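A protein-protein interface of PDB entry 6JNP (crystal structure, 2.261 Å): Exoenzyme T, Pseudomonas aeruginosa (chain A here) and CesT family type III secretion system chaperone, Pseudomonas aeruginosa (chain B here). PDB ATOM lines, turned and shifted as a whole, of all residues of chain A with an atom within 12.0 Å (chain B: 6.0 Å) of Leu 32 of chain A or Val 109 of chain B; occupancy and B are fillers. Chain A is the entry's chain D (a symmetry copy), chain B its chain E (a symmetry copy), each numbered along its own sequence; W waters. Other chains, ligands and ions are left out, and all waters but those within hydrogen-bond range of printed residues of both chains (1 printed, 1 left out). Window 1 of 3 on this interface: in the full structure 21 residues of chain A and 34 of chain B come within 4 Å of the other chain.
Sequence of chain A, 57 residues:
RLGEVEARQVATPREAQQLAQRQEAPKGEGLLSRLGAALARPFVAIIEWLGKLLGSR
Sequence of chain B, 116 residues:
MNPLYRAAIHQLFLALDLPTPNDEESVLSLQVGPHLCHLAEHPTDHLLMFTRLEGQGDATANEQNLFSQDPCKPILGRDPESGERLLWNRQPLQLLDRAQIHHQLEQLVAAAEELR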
ATOM      1  N   PRO A  26      13.183  15.707  20.936  1.00  0.00           N
ATOM      2  CA  PRO A  26      12.871  14.750  19.871  1.00  0.00           C
ATOM      3  C   PRO A  26      11.405  14.838  19.471  1.00  0.00           C
ATOM      4  O   PRO A  26      10.519  14.981  20.316  1.00  0.00           O
ATOM      5  CB  PRO A  26      13.205  13.394  20.501  1.00  0.00           C
ATOM      6  CG  PRO A  26      14.211  13.711  21.558  1.00  0.00           C
ATOM      7  CD  PRO A  26      13.817  15.057  22.097  1.00  0.00           C
ATOM      8  N   LYS A  27      11.159  14.758  18.167  1.00  0.00           N
ATOM      9  CA  LYS A  27       9.819  14.880  17.617  1.00  0.00           C
ATOM     10  C   LYS A  27       9.527  13.699  16.702  1.00  0.00           C
ATOM     11  O   LYS A  27      10.436  13.055  16.170  1.00  0.00           O
ATOM     12  CB  LYS A  27       9.644  16.198  16.850  1.00  0.00           C
ATOM     13  CG  LYS A  27      10.874  16.623  16.065  1.00  0.00           C
ATOM     14  CD  LYS A  27      10.538  17.694  15.042  1.00  0.00           C
ATOM     15  CE  LYS A  27       9.858  18.893  15.680  1.00  0.00           C
ATOM     16  NZ  LYS A  27       9.498  19.919  14.662  1.00  0.00           N
ATOM     17  N   GLY A  28       8.238  13.420  16.534  1.00  0.00           N
ATOM     18  CA  GLY A  28       7.808  12.365  15.641  1.00  0.00           C
ATOM     19  C   GLY A  28       8.041  10.958  16.138  1.00  0.00           C
ATOM     20  O   GLY A  28       8.153  10.042  15.322  1.00  0.00           O
ATOM     21  N   GLU A  29       8.118  10.753  17.452  1.00  0.00           N
ATOM     22  CA  GLU A  29       8.299   9.408  17.986  1.00  0.00           C
ATOM     23  C   GLU A  29       7.142   8.512  17.564  1.00  0.00           C
ATOM     24  O   GLU A  29       5.977   8.812  17.843  1.00  0.00           O
ATOM     25  CB  GLU A  29       8.405   9.446  19.509  1.00  0.00           C
ATOM     26  CG  GLU A  29       9.708  10.014  20.034  1.00  0.00           C
ATOM     27  CD  GLU A  29       9.890   9.752  21.515  1.00  0.00           C
ATOM     28  OE1 GLU A  29       9.316   8.763  22.020  1.00  0.00           O
ATOM     29  OE2 GLU A  29      10.603  10.537  22.175  1.00  0.00           O
ATOM     30  N   GLY A  30       7.466   7.413  16.886  1.00  0.00           N
ATOM     31  CA  GLY A  30       6.445   6.501  16.410  1.00  0.00           C
ATOM     32  C   GLY A  30       5.504   7.091  15.386  1.00  0.00           C
ATOM     33  O   GLY A  30       4.403   6.568  15.196  1.00  0.00           O
ATOM     34  N   LEU A  31       5.909   8.170  14.712  1.00  0.00           N
ATOM     35  CA  LEU A  31       5.007   8.835  13.778  1.00  0.00           C
ATOM     36  C   LEU A  31       4.836   8.031  12.495  1.00  0.00           C
ATOM     37  O   LEU A  31       3.735   7.981  11.935  1.00  0.00           O
ATOM     38  CB  LEU A  31       5.516  10.238  13.459  1.00  0.00           C
ATOM     39  CG  LEU A  31       4.637  11.013  12.476  1.00  0.00           C
ATOM     40  CD1 LEU A  31       3.257  11.247  13.065  1.00  0.00           C
ATOM     41  CD2 LEU A  31       5.288  12.320  12.100  1.00  0.00           C
ATOM     42  N   LEU A  32       5.912   7.412  12.004  1.00  0.00           N
ATOM     43  CA  LEU A  32       5.803   6.616  10.785  1.00  0.00           C
ATOM     44  C   LEU A  32       4.848   5.446  10.977  1.00  0.00           C
ATOM     45  O   LEU A  32       4.106   5.083  10.056  1.00  0.00           O
ATOM     46  CB  LEU A  32       7.181   6.119  10.348  1.00  0.00           C
ATOM     47  CG  LEU A  32       8.156   7.156   9.784  1.00  0.00           C
ATOM     48  CD1 LEU A  32       9.451   6.489   9.350  1.00  0.00           C
ATOM     49  CD2 LEU A  32       7.540   7.921   8.624  1.00  0.00           C
ATOM     50  N   SER A  33       4.845   4.845  12.169  1.00  0.00           N
ATOM     51  CA  SER A  33       3.937   3.734  12.428  1.00  0.00           C
ATOM     52  C   SER A  33       2.492   4.208  12.524  1.00  0.00           C
ATOM     53  O   SER A  33       1.573   3.509  12.079  1.00  0.00           O
ATOM     54  CB  SER A  33       4.349   3.007  13.707  1.00  0.00           C
ATOM     55  OG  SER A  33       4.319   3.877  14.823  1.00  0.00           O
ATOM     56  N   ARG A  34       2.270   5.395  13.097  1.00  0.00           N
ATOM     57  CA  ARG A  34       0.908   5.900  13.241  1.00  0.00           C
ATOM     58  C   ARG A  34       0.336   6.353  11.903  1.00  0.00           C
ATOM     59  O   ARG A  34      -0.833   6.089  11.601  1.00  0.00           O
ATOM     60  CB  ARG A  34       0.869   7.040  14.261  1.00  0.00           C
ATOM     61  CG  ARG A  34       1.160   6.590  15.685  1.00  0.00           C
ATOM     62  CD  ARG A  34       0.919   7.697  16.710  1.00  0.00           C
ATOM     63  NE  ARG A  34       2.110   8.503  16.963  1.00  0.00           N
ATOM     64  CZ  ARG A  34       2.284   9.745  16.520  1.00  0.00           C
ATOM     65  NH1 ARG A  34       1.339  10.332  15.799  1.00  0.00           N
ATOM     66  NH2 ARG A  34       3.402  10.401  16.804  1.00  0.00           N
ATOM     67  N   LEU A  35       1.140   7.033  11.085  1.00  0.00           N
ATOM     68  CA  LEU A  35       0.655   7.502   9.792  1.00  0.00           C
ATOM     69  C   LEU A  35       0.709   6.411   8.731  1.00  0.00           C
ATOM     70  O   LEU A  35      -0.050   6.464   7.758  1.00  0.00           O
ATOM     71  CB  LEU A  35       1.459   8.719   9.330  1.00  0.00           C
ATOM     72  CG  LEU A  35       1.230  10.018  10.093  1.00  0.00           C
ATOM     73  CD1 LEU A  35       2.094  11.124   9.515  1.00  0.00           C
ATOM     74  CD2 LEU A  35      -0.239  10.413  10.059  1.00  0.00           C
ATOM     75  N   GLY A  36       1.585   5.429   8.888  1.00  0.00           N
ATOM     76  CA  GLY A  36       1.740   4.389   7.896  1.00  0.00           C
ATOM     77  C   GLY A  36       2.489   4.865   6.663  1.00  0.00           C
ATOM     78  O   GLY A  36       2.634   6.055   6.405  1.00  0.00           O
ATOM     79  N   ALA A  37       2.966   3.897   5.889  1.00  0.00           N
ATOM     80  CA  ALA A  37       3.770   4.183   4.713  1.00  0.00           C
ATOM     81  C   ALA A  37       3.373   3.235   3.595  1.00  0.00           C
ATOM     82  O   ALA A  37       3.103   2.059   3.838  1.00  0.00           O
ATOM     83  CB  ALA A  37       5.270   4.052   5.010  1.00  0.00           C
ATOM     84  N   ALA A  38       3.324   3.763   2.376  1.00  0.00           N
ATOM     85  CA  ALA A  38       3.034   2.974   1.190  1.00  0.00           C
ATOM     86  C   ALA A  38       3.799   3.580   0.028  1.00  0.00           C
ATOM     87  O   ALA A  38       4.067   4.786   0.006  1.00  0.00           O
ATOM     88  CB  ALA A  38       1.531   2.938   0.883  1.00  0.00           C
ATOM     89  N   LEU A  39       4.165   2.735  -0.930  1.00  0.00           N
ATOM     90  CA  LEU A  39       4.824   3.225  -2.130  1.00  0.00           C
ATOM     91  C   LEU A  39       3.824   4.002  -2.975  1.00  0.00           C
ATOM     92  O   LEU A  39       2.692   3.554  -3.185  1.00  0.00           O
ATOM     93  CB  LEU A  39       5.422   2.068  -2.930  1.00  0.00           C
ATOM     94  CG  LEU A  39       6.526   2.395  -3.943  1.00  0.00           C
ATOM     95  CD1 LEU A  39       7.445   1.196  -4.117  1.00  0.00           C
ATOM     96  CD2 LEU A  39       5.950   2.820  -5.287  1.00  0.00           C
ATOM     97  N   ALA A  40       4.238   5.168  -3.455  1.00  0.00           N
ATOM     98  CA  ALA A  40       3.374   6.044  -4.230  1.00  0.00           C
ATOM     99  C   ALA A  40       3.865   6.123  -5.668  1.00  0.00           C
ATOM    100  O   ALA A  40       5.074   6.141  -5.924  1.00  0.00           O
ATOM    101  CB  ALA A  40       3.322   7.447  -3.619  1.00  0.00           C
ATOM    102  N   LEU B  12      15.339   0.492   4.475  1.00  0.00           N
ATOM    103  CA  LEU B  12      14.190   1.348   4.764  1.00  0.00           C
ATOM    104  C   LEU B  12      12.879   0.619   4.499  1.00  0.00           C
ATOM    105  O   LEU B  12      11.951   0.668   5.315  1.00  0.00           O
ATOM    106  CB  LEU B  12      14.256   2.629   3.934  1.00  0.00           C
ATOM    107  CG  LEU B  12      13.057   3.569   4.092  1.00  0.00           C
ATOM    108  CD1 LEU B  12      12.892   3.995   5.545  1.00  0.00           C
ATOM    109  CD2 LEU B  12      13.199   4.781   3.191  1.00  0.00           C
ATOM    110  N   LEU B  16       9.638  -0.529   6.908  1.00  0.00           N
ATOM    111  CA  LEU B  16       8.297  -0.019   6.651  1.00  0.00           C
ATOM    112  C   LEU B  16       7.313  -1.112   6.254  1.00  0.00           C
ATOM    113  O   LEU B  16       6.182  -0.797   5.867  1.00  0.00           O
ATOM    114  CB  LEU B  16       8.345   1.059   5.566  1.00  0.00           C
ATOM    115  CG  LEU B  16       9.092   2.349   5.908  1.00  0.00           C
ATOM    116  CD1 LEU B  16       9.276   3.202   4.665  1.00  0.00           C
ATOM    117  CD2 LEU B  16       8.347   3.123   6.984  1.00  0.00           C
ATOM    118  N   VAL B  32       3.211   8.807   3.131  1.00  0.00           N
ATOM    119  CA  VAL B  32       3.201   8.702   4.584  1.00  0.00           C
ATOM    120  C   VAL B  32       2.044   9.563   5.071  1.00  0.00           C
ATOM    121  O   VAL B  32       2.180  10.783   5.217  1.00  0.00           O
ATOM    122  CB  VAL B  32       4.532   9.144   5.203  1.00  0.00           C
ATOM    123  CG1 VAL B  32       4.532   8.875   6.698  1.00  0.00           C
ATOM    124  CG2 VAL B  32       5.692   8.440   4.519  1.00  0.00           C
ATOM    125  N   HIS B  35       1.374  12.939   3.420  1.00  0.00           N
ATOM    126  CA  HIS B  35       2.636  13.525   2.990  1.00  0.00           C
ATOM    127  C   HIS B  35       3.253  12.676   1.885  1.00  0.00           C
ATOM    128  O   HIS B  35       3.577  11.501   2.101  1.00  0.00           O
ATOM    129  CB  HIS B  35       3.596  13.657   4.171  1.00  0.00           C
ATOM    130  CG  HIS B  35       3.013  14.392   5.335  1.00  0.00           C
ATOM    131  ND1 HIS B  35       2.910  15.766   5.371  1.00  0.00           N
ATOM    132  CD2 HIS B  35       2.492  13.944   6.502  1.00  0.00           C
ATOM    133  CE1 HIS B  35       2.357  16.133   6.512  1.00  0.00           C
ATOM    134  NE2 HIS B  35       2.092  15.047   7.216  1.00  0.00           N
ATOM    135  N   CYS B  37       6.354  11.874   0.095  1.00  0.00           N
ATOM    136  CA  CYS B  37       7.788  11.997   0.304  1.00  0.00           C
ATOM    137  C   CYS B  37       8.538  11.352  -0.855  1.00  0.00           C
ATOM    138  O   CYS B  37       8.067  10.389  -1.461  1.00  0.00           O
ATOM    139  CB  CYS B  37       8.203  11.350   1.629  1.00  0.00           C
ATOM    140  SG  CYS B  37       7.257  11.949   3.055  1.00  0.00           S
ATOM    141  N   ILE B 101      18.031   5.364   8.729  1.00  0.00           N
ATOM    142  CA  ILE B 101      17.233   5.770   7.576  1.00  0.00           C
ATOM    143  C   ILE B 101      15.763   5.911   7.968  1.00  0.00           C
ATOM    144  O   ILE B 101      15.064   6.836   7.517  1.00  0.00           O
ATOM    145  CB  ILE B 101      17.450   4.780   6.412  1.00  0.00           C
ATOM    146  CG1 ILE B 101      16.832   5.304   5.121  1.00  0.00           C
ATOM    147  CG2 ILE B 101      16.907   3.394   6.739  1.00  0.00           C
ATOM    148  CD1 ILE B 101      17.178   4.457   3.924  1.00  0.00           C
ATOM    149  N   HIS B 102      15.280   5.019   8.841  1.00  0.00           N
ATOM    150  CA  HIS B 102      13.933   5.180   9.378  1.00  0.00           C
ATOM    151  C   HIS B 102      13.810   6.489  10.149  1.00  0.00           C
ATOM    152  O   HIS B 102      12.802   7.196  10.031  1.00  0.00           O
ATOM    153  CB  HIS B 102      13.581   3.991  10.271  1.00  0.00           C
ATOM    154  CG  HIS B 102      12.193   4.045  10.827  1.00  0.00           C
ATOM    155  ND1 HIS B 102      11.868   4.784  11.944  1.00  0.00           N
ATOM    156  CD2 HIS B 102      11.045   3.451  10.422  1.00  0.00           C
ATOM    157  CE1 HIS B 102      10.579   4.645  12.201  1.00  0.00           C
ATOM    158  NE2 HIS B 102      10.057   3.839  11.295  1.00  0.00           N
ATOM    159  N   HIS B 103      14.838   6.834  10.929  1.00  0.00           N
ATOM    160  CA  HIS B 103      14.824   8.086  11.678  1.00  0.00           C
ATOM    161  C   HIS B 103      14.808   9.290  10.745  1.00  0.00           C
ATOM    162  O   HIS B 103      14.126  10.284  11.013  1.00  0.00           O
ATOM    163  CB  HIS B 103      16.033   8.140  12.609  1.00  0.00           C
ATOM    164  CG  HIS B 103      16.119   9.396  13.417  1.00  0.00           C
ATOM    165  ND1 HIS B 103      15.436   9.566  14.601  1.00  0.00           N
ATOM    166  CD2 HIS B 103      16.808  10.543  13.211  1.00  0.00           C
ATOM    167  CE1 HIS B 103      15.699  10.765  15.091  1.00  0.00           C
ATOM    168  NE2 HIS B 103      16.528  11.378  14.266  1.00  0.00           N
ATOM    169  N   GLN B 104      15.568   9.222   9.649  1.00  0.00           N
ATOM    170  CA  GLN B 104      15.575  10.311   8.676  1.00  0.00           C
ATOM    171  C   GLN B 104      14.181  10.539   8.104  1.00  0.00           C
ATOM    172  O   GLN B 104      13.674  11.674   8.087  1.00  0.00           O
ATOM    173  CB  GLN B 104      16.577  10.001   7.561  1.00  0.00           C
ATOM    174  CG  GLN B 104      16.720  11.099   6.516  1.00  0.00           C
ATOM    175  CD  GLN B 104      17.700  10.740   5.412  1.00  0.00           C
ATOM    176  OE1 GLN B 104      18.360   9.701   5.462  1.00  0.00           O
ATOM    177  NE2 GLN B 104      17.799  11.602   4.409  1.00  0.00           N
ATOM    178  N   LEU B 105      13.540   9.462   7.637  1.00  0.00           N
ATOM    179  CA  LEU B 105      12.189   9.604   7.099  1.00  0.00           C
ATOM    180  C   LEU B 105      11.223  10.124   8.157  1.00  0.00           C
ATOM    181  O   LEU B 105      10.370  10.977   7.868  1.00  0.00           O
ATOM    182  CB  LEU B 105      11.690   8.274   6.535  1.00  0.00           C
ATOM    183  CG  LEU B 105      10.261   8.338   5.979  1.00  0.00           C
ATOM    184  CD1 LEU B 105      10.149   9.419   4.912  1.00  0.00           C
ATOM    185  CD2 LEU B 105       9.817   6.991   5.428  1.00  0.00           C
ATOM    186  N   GLU B 106      11.345   9.631   9.391  1.00  0.00           N
ATOM    187  CA  GLU B 106      10.408  10.032  10.432  1.00  0.00           C
ATOM    188  C   GLU B 106      10.575  11.500  10.793  1.00  0.00           C
ATOM    189  O   GLU B 106       9.589  12.193  11.053  1.00  0.00           O
ATOM    190  CB  GLU B 106      10.579   9.151  11.665  1.00  0.00           C
ATOM    191  CG  GLU B 106       9.368   9.165  12.576  1.00  0.00           C
ATOM    192  CD  GLU B 106       9.366   8.017  13.562  1.00  0.00           C
ATOM    193  OE1 GLU B 106      10.338   7.897  14.337  1.00  0.00           O
ATOM    194  OE2 GLU B 106       8.392   7.234  13.557  1.00  0.00           O
ATOM    195  N   GLN B 107      11.813  11.997  10.808  1.00  0.00           N
ATOM    196  CA  GLN B 107      12.033  13.412  11.086  1.00  0.00           C
ATOM    197  C   GLN B 107      11.478  14.282   9.966  1.00  0.00           C
ATOM    198  O   GLN B 107      10.865  15.330  10.229  1.00  0.00           O
ATOM    199  CB  GLN B 107      13.522  13.682  11.293  1.00  0.00           C
ATOM    200  CG  GLN B 107      14.070  13.091  12.576  1.00  0.00           C
ATOM    201  CD  GLN B 107      13.316  13.574  13.797  1.00  0.00           C
ATOM    202  OE1 GLN B 107      13.245  14.774  14.060  1.00  0.00           O
ATOM    203  NE2 GLN B 107      12.735  12.642  14.543  1.00  0.00           N
ATOM    204  N   LEU B 108      11.684  13.865   8.712  1.00  0.00           N
ATOM    205  CA  LEU B 108      11.074  14.583   7.597  1.00  0.00           C
ATOM    206  C   LEU B 108       9.561  14.670   7.767  1.00  0.00           C
ATOM    207  O   LEU B 108       8.966  15.751   7.653  1.00  0.00           O
ATOM    208  CB  LEU B 108      11.425  13.903   6.275  1.00  0.00           C
ATOM    209  CG  LEU B 108      10.779  14.554   5.053  1.00  0.00           C
ATOM    210  CD1 LEU B 108      11.262  15.985   4.926  1.00  0.00           C
ATOM    211  CD2 LEU B 108      11.069  13.768   3.785  1.00  0.00           C
ATOM    212  N   VAL B 109       8.923  13.534   8.060  1.00  0.00           N
ATOM    213  CA  VAL B 109       7.468  13.513   8.171  1.00  0.00           C
ATOM    214  C   VAL B 109       6.998  14.306   9.388  1.00  0.00           C
ATOM    215  O   VAL B 109       5.931  14.927   9.354  1.00  0.00           O
ATOM    216  CB  VAL B 109       6.957  12.061   8.201  1.00  0.00           C
ATOM    217  CG1 VAL B 109       5.452  12.024   8.401  1.00  0.00           C
ATOM    218  CG2 VAL B 109       7.329  11.351   6.911  1.00  0.00           C
ATOM    219  N   ALA B 110       7.775  14.313  10.472  1.00  0.00           N
ATOM    220  CA  ALA B 110       7.389  15.086  11.649  1.00  0.00           C
ATOM    221  C   ALA B 110       7.398  16.576  11.344  1.00  0.00           C
ATOM    222  O   ALA B 110       6.454  17.302  11.686  1.00  0.00           O
ATOM    223  CB  ALA B 110       8.320  14.765  12.818  1.00  0.00           C
ATOM    224  N   ALA B 111       8.459  17.052  10.689  1.00  0.00           N
ATOM    225  CA  ALA B 111       8.488  18.462  10.318  1.00  0.00           C
ATOM    226  C   ALA B 111       7.401  18.794   9.303  1.00  0.00           C
ATOM    227  O   ALA B 111       6.891  19.921   9.292  1.00  0.00           O
ATOM    228  CB  ALA B 111       9.862  18.842   9.778  1.00  0.00           C
ATOM    229  N   ALA B 112       7.033  17.836   8.448  1.00  0.00           N
ATOM    230  CA  ALA B 112       5.915  18.064   7.537  1.00  0.00           C
ATOM    231  C   ALA B 112       4.600  18.184   8.300  1.00  0.00           C
ATOM    232  O   ALA B 112       3.760  19.032   7.975  1.00  0.00           O
ATOM    233  CB  ALA B 112       5.841  16.941   6.504  1.00  0.00           C
ATOM    234  N   GLU B 113       4.406  17.338   9.315  1.00  0.00           N
ATOM    235  CA  GLU B 113       3.211  17.409  10.149  1.00  0.00           C
ATOM    236  C   GLU B 113       3.154  18.708  10.939  1.00  0.00           C
ATOM    237  O   GLU B 113       2.062  19.180  11.272  1.00  0.00           O
ATOM    238  CB  GLU B 113       3.168  16.217  11.108  1.00  0.00           C
ATOM    239  CG  GLU B 113       2.687  14.923  10.483  1.00  0.00           C
ATOM    240  CD  GLU B 113       1.175  14.803  10.493  1.00  0.00           C
ATOM    241  OE1 GLU B 113       0.607  14.516  11.569  1.00  0.00           O
ATOM    242  OE2 GLU B 113       0.557  15.007   9.428  1.00  0.00           O
ATOM    243  N   GLU B 114       4.312  19.287  11.262  1.00  0.00           N
ATOM    244  CA  GLU B 114       4.313  20.521  12.040  1.00  0.00           C
ATOM    245  C   GLU B 114       3.819  21.707  11.222  1.00  0.00           C
ATOM    246  O   GLU B 114       3.181  22.613  11.770  1.00  0.00           O
ATOM    247  CB  GLU B 114       5.713  20.787  12.589  1.00  0.00           C
ATOM    248  CG  GLU B 114       5.796  21.949  13.561  1.00  0.00           C
ATOM    249  CD  GLU B 114       6.869  21.744  14.611  1.00  0.00           C
ATOM    250  OE1 GLU B 114       7.066  20.586  15.038  1.00  0.00           O
ATOM    251  OE2 GLU B 114       7.519  22.735  15.006  1.00  0.00           O
HETATM  252  O   HOH W   1      10.136   6.346  16.260  1.00  0.00           O
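O of Lys 27 of chain A is in hydrogen-bond range of NE2 of Gln 107 of chain B (2.8 Å).
O of Gly 28 of chain A lies close to OE1 of Glu 106 of chain B, 3.2 Å away.
OE2 of Glu 106 of chain B sits at hydrogen-bond distance from N of Leu 32 of chain A, 2.9 Å away.
The side-chain carboxylate of Glu 106 of chain B lies within hydrogen-bond range of the backbone NH of Leu 31 of chain A (2.9 Å).
The backbone NH (N) of Gly 30 of chain A sits close to the side-chain carboxylate (OE2) of Glu 106 of chain B, at 3.5 Å.
OE1 of Glu 114 of chain B is in salt-bridge range of NZ of Lys 27 of chain A.
A ring nitrogen (NE2) of His 35 of chain B sits at hydrogen-bond distance from the side-chain carboxylate (OE2) of Glu 113 of chain B (2.7 Å).
The backbone carbonyl oxygen of Gly 30 of chain A lies close to the guanidinium group of Arg 34 of chain A (3.5 Å).
The backbone carbonyl oxygen of Gly 30 of chain A lies within hydrogen-bond range of the side-chain hydroxyl of Ser 33 of chain A, 2.7 Å away.
Among the printed residues, merely in contact across the chains: Gly 36 of chain A with Val 32 of chain B, Leu 32 of chain A with His 102 of chain B, Leu 31 of chain A with Ala 110 of chain B, Leu 35 of chain A with Val 109 of chain B, Leu 32 of chain A with Val 32 of chain B, Leu 31 of chain A with Val 109 of chain B, Gly 28 of chain A with Ala 110 of chain B, Ala 37 of chain A with Leu 16 of chain B, Leu 32 of chain A with Leu 105 of chain B, Leu 32 of chain A with Val 109 of chain B and Leu 35 of chain A with Glu 113 of chain B.
Pro 26 of chain A touches none of the printed residues of chain B.
Of the printed residues of chain B, Leu 31 of chain A touches Glu 106, Val 109 and Ala 110.
Leu 32 of chain A touches five residues of chain B.
Printed residues of chain B within 4 Å of Leu 35 of chain A: Val 109 and Glu 113.
Leu 16 of chain B touches one residue of chain A.
No residue of chain A comes within 4 Å of His 35 of chain B.
Printed residues of chain A within 4 Å of Leu 105 of chain B: Leu 32 (3.8 Å).
Of chain A, only Gly 28 (2.9 Å), Gly 30 (3.4 Å), Leu 31 (2.9 Å) and Leu 32 (2.9 Å) come within 4 Å of Glu 106 of chain B.
Gln 107 of chain B touches just one residue of chain A: Lys 27.
No residue of chain A comes within 4 Å of Leu 108 of chain B.
Val 109 of chain B touches three residues of chain A.
Of the printed residues of chain A, Ala 110 of chain B touches Gly 28 and Leu 31.
No residue of chain A comes within 4 Å of Ala 111 of chain B.
Of the printed residues of chain A, Glu 113 of chain B touches Leu 35 (3.9 Å).
Printed residues of chain A within 4 Å of Glu 114 of chain B: Lys 27 (2.5 Å).
The nearest residue of chain B that does not touch Leu 32 of chain A is Leu 16 of chain B (4.3 Å).
The nearest printed residue of chain B that does not touch Leu 35 of chain A is Val 32 of chain B (4.05 Å).
Of the 15 printed residues of chain A, 8 touch a printed residue of chain B.
Hydrophobic or aromatic side chains of chain A within 4 Å of the printed part of chain B: Leu 31, Leu 32, Leu 35 and Ala 37.
Hydrophobic or aromatic side chains of chain B within 4 Å of the printed part of chain A: Leu 16, Val 32, His 102, Leu 105, Val 109 and Ala 110.
Among the printed residues, Asp or Glu carboxylates within 4 Å of a Lys or Arg side-chain nitrogen of the other chain: Lys 27 of chain A with Glu 114 of chain B.
Water W1 lies within hydrogen-bond range of OE1 of Glu 106 of chain B and N of Gly 30 of chain A.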
